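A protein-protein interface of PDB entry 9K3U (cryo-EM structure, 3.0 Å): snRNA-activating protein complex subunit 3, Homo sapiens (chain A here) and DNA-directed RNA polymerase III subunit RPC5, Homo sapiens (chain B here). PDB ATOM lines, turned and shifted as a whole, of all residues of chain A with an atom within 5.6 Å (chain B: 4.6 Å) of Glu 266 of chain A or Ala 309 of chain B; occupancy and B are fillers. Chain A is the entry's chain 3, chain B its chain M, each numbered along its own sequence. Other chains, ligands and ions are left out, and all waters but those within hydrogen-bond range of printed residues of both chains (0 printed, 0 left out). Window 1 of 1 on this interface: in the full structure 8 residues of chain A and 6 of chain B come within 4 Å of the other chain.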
ATOM      1  N   LEU A 246      28.317  -3.000 -32.367  1.00  0.00           N
ATOM      2  CA  LEU A 246      27.002  -2.386 -32.539  1.00  0.00           C
ATOM      3  C   LEU A 246      25.983  -2.966 -31.561  1.00  0.00           C
ATOM      4  O   LEU A 246      25.416  -2.240 -30.736  1.00  0.00           O
ATOM      5  CB  LEU A 246      26.524  -2.563 -33.983  1.00  0.00           C
ATOM      6  CG  LEU A 246      27.272  -1.763 -35.053  1.00  0.00           C
ATOM      7  CD1 LEU A 246      26.708  -2.066 -36.433  1.00  0.00           C
ATOM      8  CD2 LEU A 246      27.205  -0.270 -34.761  1.00  0.00           C
ATOM      9  N   LYS A 248      25.540  -4.448 -28.587  1.00  0.00           N
ATOM     10  CA  LYS A 248      26.099  -4.741 -27.273  1.00  0.00           C
ATOM     11  C   LYS A 248      25.082  -5.354 -26.320  1.00  0.00           C
ATOM     12  O   LYS A 248      25.445  -5.684 -25.185  1.00  0.00           O
ATOM     13  CB  LYS A 248      26.675  -3.462 -26.659  1.00  0.00           C
ATOM     14  CG  LYS A 248      27.893  -2.922 -27.389  1.00  0.00           C
ATOM     15  CD  LYS A 248      28.397  -1.631 -26.761  1.00  0.00           C
ATOM     16  CE  LYS A 248      29.696  -1.160 -27.404  1.00  0.00           C
ATOM     17  NZ  LYS A 248      30.793  -2.158 -27.263  1.00  0.00           N
ATOM     18  N   SER A 249      23.832  -5.517 -26.745  1.00  0.00           N
ATOM     19  CA  SER A 249      22.811  -6.087 -25.879  1.00  0.00           C
ATOM     20  C   SER A 249      23.078  -7.567 -25.644  1.00  0.00           C
ATOM     21  O   SER A 249      23.249  -8.336 -26.593  1.00  0.00           O
ATOM     22  CB  SER A 249      21.428  -5.889 -26.496  1.00  0.00           C
ATOM     23  OG  SER A 249      21.156  -4.515 -26.711  1.00  0.00           O
ATOM     24  N   TYR A 264      28.098  -0.751 -20.733  1.00  0.00           N
ATOM     25  CA  TYR A 264      28.245   0.159 -21.851  1.00  0.00           C
ATOM     26  C   TYR A 264      26.978   0.985 -22.034  1.00  0.00           C
ATOM     27  O   TYR A 264      25.874   0.481 -21.804  1.00  0.00           O
ATOM     28  CB  TYR A 264      28.541  -0.618 -23.142  1.00  0.00           C
ATOM     29  CG  TYR A 264      29.675  -1.608 -23.006  1.00  0.00           C
ATOM     30  CD1 TYR A 264      30.841  -1.271 -22.328  1.00  0.00           C
ATOM     31  CD2 TYR A 264      29.580  -2.884 -23.545  1.00  0.00           C
ATOM     32  CE1 TYR A 264      31.877  -2.174 -22.196  1.00  0.00           C
ATOM     33  CE2 TYR A 264      30.613  -3.793 -23.419  1.00  0.00           C
ATOM     34  CZ  TYR A 264      31.759  -3.434 -22.744  1.00  0.00           C
ATOM     35  OH  TYR A 264      32.790  -4.338 -22.617  1.00  0.00           O
ATOM     36  N   PRO A 265      27.097   2.252 -22.439  1.00  0.00           N
ATOM     37  CA  PRO A 265      25.913   3.105 -22.596  1.00  0.00           C
ATOM     38  C   PRO A 265      25.094   2.837 -23.850  1.00  0.00           C
ATOM     39  O   PRO A 265      24.184   3.618 -24.143  1.00  0.00           O
ATOM     40  CB  PRO A 265      26.521   4.516 -22.638  1.00  0.00           C
ATOM     41  CG  PRO A 265      27.871   4.321 -23.212  1.00  0.00           C
ATOM     42  CD  PRO A 265      28.345   2.992 -22.698  1.00  0.00           C
ATOM     43  N   GLU A 266      25.379   1.767 -24.598  1.00  0.00           N
ATOM     44  CA  GLU A 266      24.629   1.432 -25.803  1.00  0.00           C
ATOM     45  C   GLU A 266      23.897   0.099 -25.670  1.00  0.00           C
ATOM     46  O   GLU A 266      23.465  -0.468 -26.679  1.00  0.00           O
ATOM     47  CB  GLU A 266      25.552   1.400 -27.022  1.00  0.00           C
ATOM     48  CG  GLU A 266      26.390   2.653 -27.216  1.00  0.00           C
ATOM     49  CD  GLU A 266      27.646   2.649 -26.367  1.00  0.00           C
ATOM     50  OE1 GLU A 266      28.596   3.385 -26.706  1.00  0.00           O
ATOM     51  OE2 GLU A 266      27.683   1.905 -25.365  1.00  0.00           O
ATOM     52  N   CYS A 267      23.752  -0.413 -24.451  1.00  0.00           N
ATOM     53  CA  CYS A 267      23.094  -1.691 -24.222  1.00  0.00           C
ATOM     54  C   CYS A 267      21.616  -1.468 -23.932  1.00  0.00           C
ATOM     55  O   CYS A 267      21.258  -0.704 -23.031  1.00  0.00           O
ATOM     56  CB  CYS A 267      23.753  -2.434 -23.061  1.00  0.00           C
ATOM     57  SG  CYS A 267      25.486  -2.870 -23.342  1.00  0.00           S
ATOM     58  N   ARG A 268      20.760  -2.141 -24.699  1.00  0.00           N
ATOM     59  CA  ARG A 268      19.323  -2.076 -24.497  1.00  0.00           C
ATOM     60  C   ARG A 268      18.913  -3.136 -23.477  1.00  0.00           C
ATOM     61  O   ARG A 268      19.755  -3.772 -22.836  1.00  0.00           O
ATOM     62  CB  ARG A 268      18.601  -2.245 -25.835  1.00  0.00           C
ATOM     63  CG  ARG A 268      18.776  -1.062 -26.776  1.00  0.00           C
ATOM     64  CD  ARG A 268      18.275  -1.379 -28.174  1.00  0.00           C
ATOM     65  NE  ARG A 268      19.123  -2.356 -28.849  1.00  0.00           N
ATOM     66  CZ  ARG A 268      18.932  -2.781 -30.092  1.00  0.00           C
ATOM     67  NH1 ARG A 268      17.915  -2.321 -30.813  1.00  0.00           N
ATOM     68  NH2 ARG A 268      19.760  -3.674 -30.621  1.00  0.00           N
ATOM     69  N   LEU B 278      20.122   4.936 -25.169  1.00  0.00           N
ATOM     70  CA  LEU B 278      20.654   6.015 -25.997  1.00  0.00           C
ATOM     71  C   LEU B 278      20.111   5.942 -27.419  1.00  0.00           C
ATOM     72  O   LEU B 278      19.794   6.973 -28.024  1.00  0.00           O
ATOM     73  CB  LEU B 278      22.183   5.958 -26.004  1.00  0.00           C
ATOM     74  CG  LEU B 278      22.900   7.026 -26.833  1.00  0.00           C
ATOM     75  CD1 LEU B 278      22.561   8.420 -26.329  1.00  0.00           C
ATOM     76  CD2 LEU B 278      24.402   6.797 -26.813  1.00  0.00           C
ATOM     77  N   ASP B 306      29.083   9.125 -24.278  1.00  0.00           N
ATOM     78  CA  ASP B 306      30.261   9.198 -25.128  1.00  0.00           C
ATOM     79  C   ASP B 306      29.910   9.741 -26.509  1.00  0.00           C
ATOM     80  O   ASP B 306      28.866   9.419 -27.089  1.00  0.00           O
ATOM     81  CB  ASP B 306      30.905   7.820 -25.259  1.00  0.00           C
ATOM     82  CG  ASP B 306      32.302   7.884 -25.846  1.00  0.00           C
ATOM     83  OD1 ASP B 306      33.214   8.391 -25.160  1.00  0.00           O
ATOM     84  OD2 ASP B 306      32.490   7.428 -26.993  1.00  0.00           O
ATOM     85  N   SER B 307      30.806  10.580 -27.037  1.00  0.00           N
ATOM     86  CA  SER B 307      30.597  11.151 -28.363  1.00  0.00           C
ATOM     87  C   SER B 307      30.578  10.075 -29.439  1.00  0.00           C
ATOM     88  O   SER B 307      29.788  10.162 -30.384  1.00  0.00           O
ATOM     89  CB  SER B 307      31.682  12.185 -28.666  1.00  0.00           C
ATOM     90  OG  SER B 307      32.970  11.594 -28.637  1.00  0.00           O
ATOM     91  N   VAL B 308      31.429   9.054 -29.316  1.00  0.00           N
ATOM     92  CA  VAL B 308      31.425   7.972 -30.295  1.00  0.00           C
ATOM     93  C   VAL B 308      30.103   7.215 -30.240  1.00  0.00           C
ATOM     94  O   VAL B 308      29.559   6.815 -31.275  1.00  0.00           O
ATOM     95  CB  VAL B 308      32.624   7.035 -30.064  1.00  0.00           C
ATOM     96  CG1 VAL B 308      32.669   5.952 -31.136  1.00  0.00           C
ATOM     97  CG2 VAL B 308      33.924   7.826 -30.040  1.00  0.00           C
ATOM     98  N   ALA B 309      29.565   7.011 -29.038  1.00  0.00           N
ATOM     99  CA  ALA B 309      28.272   6.345 -28.914  1.00  0.00           C
ATOM    100  C   ALA B 309      27.167   7.178 -29.548  1.00  0.00           C
ATOM    101  O   ALA B 309      26.317   6.646 -30.273  1.00  0.00           O
ATOM    102  CB  ALA B 309      27.962   6.074 -27.441  1.00  0.00           C
ATOM    103  N   VAL B 310      27.160   8.488 -29.288  1.00  0.00           N
ATOM    104  CA  VAL B 310      26.149   9.352 -29.889  1.00  0.00           C
ATOM    105  C   VAL B 310      26.270   9.336 -31.407  1.00  0.00           C
ATOM    106  O   VAL B 310      25.264   9.338 -32.126  1.00  0.00           O
ATOM    107  CB  VAL B 310      26.267  10.780 -29.324  1.00  0.00           C
ATOM    108  CG1 VAL B 310      25.256  11.705 -29.992  1.00  0.00           C
ATOM    109  CG2 VAL B 310      26.072  10.769 -27.813  1.00  0.00           C
ATOM    110  N   LEU B 311      27.503   9.317 -31.919  1.00  0.00           N
ATOM    111  CA  LEU B 311      27.707   9.275 -33.362  1.00  0.00           C
ATOM    112  C   LEU B 311      27.183   7.970 -33.952  1.00  0.00           C
ATOM    113  O   LEU B 311      26.514   7.973 -34.991  1.00  0.00           O
ATOM    114  CB  LEU B 311      29.193   9.448 -33.682  1.00  0.00           C
ATOM    115  CG  LEU B 311      29.593   9.386 -35.158  1.00  0.00           C
ATOM    116  CD1 LEU B 311      28.946  10.519 -35.940  1.00  0.00           C
ATOM    117  CD2 LEU B 311      31.107   9.429 -35.299  1.00  0.00           C
ATOM    118  N   ARG B 312      27.496   6.841 -33.311  1.00  0.00           N
ATOM    119  CA  ARG B 312      27.010   5.556 -33.801  1.00  0.00           C
ATOM    120  C   ARG B 312      25.490   5.489 -33.745  1.00  0.00           C
ATOM    121  O   ARG B 312      24.859   4.838 -34.586  1.00  0.00           O
ATOM    122  CB  ARG B 312      27.630   4.420 -32.990  1.00  0.00           C
ATOM    123  CG  ARG B 312      29.123   4.247 -33.217  1.00  0.00           C
ATOM    124  CD  ARG B 312      29.698   3.145 -32.341  1.00  0.00           C
ATOM    125  NE  ARG B 312      29.593   3.463 -30.921  1.00  0.00           N
ATOM    126  CZ  ARG B 312      30.009   2.666 -29.942  1.00  0.00           C
ATOM    127  NH1 ARG B 312      30.564   1.495 -30.222  1.00  0.00           N
ATOM    128  NH2 ARG B 312      29.869   3.041 -28.678  1.00  0.00           N
ATOM    129  N   GLY B 313      24.886   6.154 -32.762  1.00  0.00           N
ATOM    130  CA  GLY B 313      23.436   6.141 -32.662  1.00  0.00           C
ATOM    131  C   GLY B 313      22.770   7.027 -33.698  1.00  0.00           C
ATOM    132  O   GLY B 313      21.708   6.687 -34.226  1.00  0.00           O
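Among the printed residues, merely in contact across the chains: Glu 266 of chain A with Ala 309 of chain B, Pro 265 of chain A with Leu 278 of chain B and Lys 248 of chain A with Arg 312 of chain B.
Of the printed residues of chain B, Lys 248 of chain A touches Arg 312 (3.97 Å).
Glu 266 of chain A touches two residues of chain B.
Of chain A, only Glu 266 comes within 4 Å of Ala 309 of chain B.
Of the printed residues of chain A, Arg 312 of chain B touches Lys 248 (3.97 Å) and Glu 266 (2.4 Å).
The nearest printed residue of chain B that does not touch Glu 266 of chain A is Leu 278 of chain B (4.6 Å).
The nearest residue of chain A that does not touch Ala 309 of chain B is Pro 265 of chain A (4.6 Å).
Of the 9 printed residues of chain B, 3 touch a printed residue of chain A.
Printed residues of chain B that touch a printed residue of chain A: Leu 278, Ala 309 and Arg 312.
Printed residues of chain A that touch a printed residue of chain B: Lys 248, Pro 265 and Glu 266.
Among the printed residues, 4 pairs touch across the chains.
Among the printed residues, Asp or Glu carboxylates within 4 Å of a Lys or Arg side-chain nitrogen of the other chain: Glu 266 of chain A with Arg 312 of chain B.
The side-chain carboxylate (OE1) of Glu 266 of chain A lies close to the guanidinium group (NH2) of Arg 312 of chain B.
The backbone carbonyl oxygen (O) of Lys 248 of chain A sits at hydrogen-bond distance from the side-chain sulfur (SG) of Cys 267 of chain A, at 3.4 Å.
NE of Arg 312 of chain B lies close to O of Val 308 of chain B (3.4 Å).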
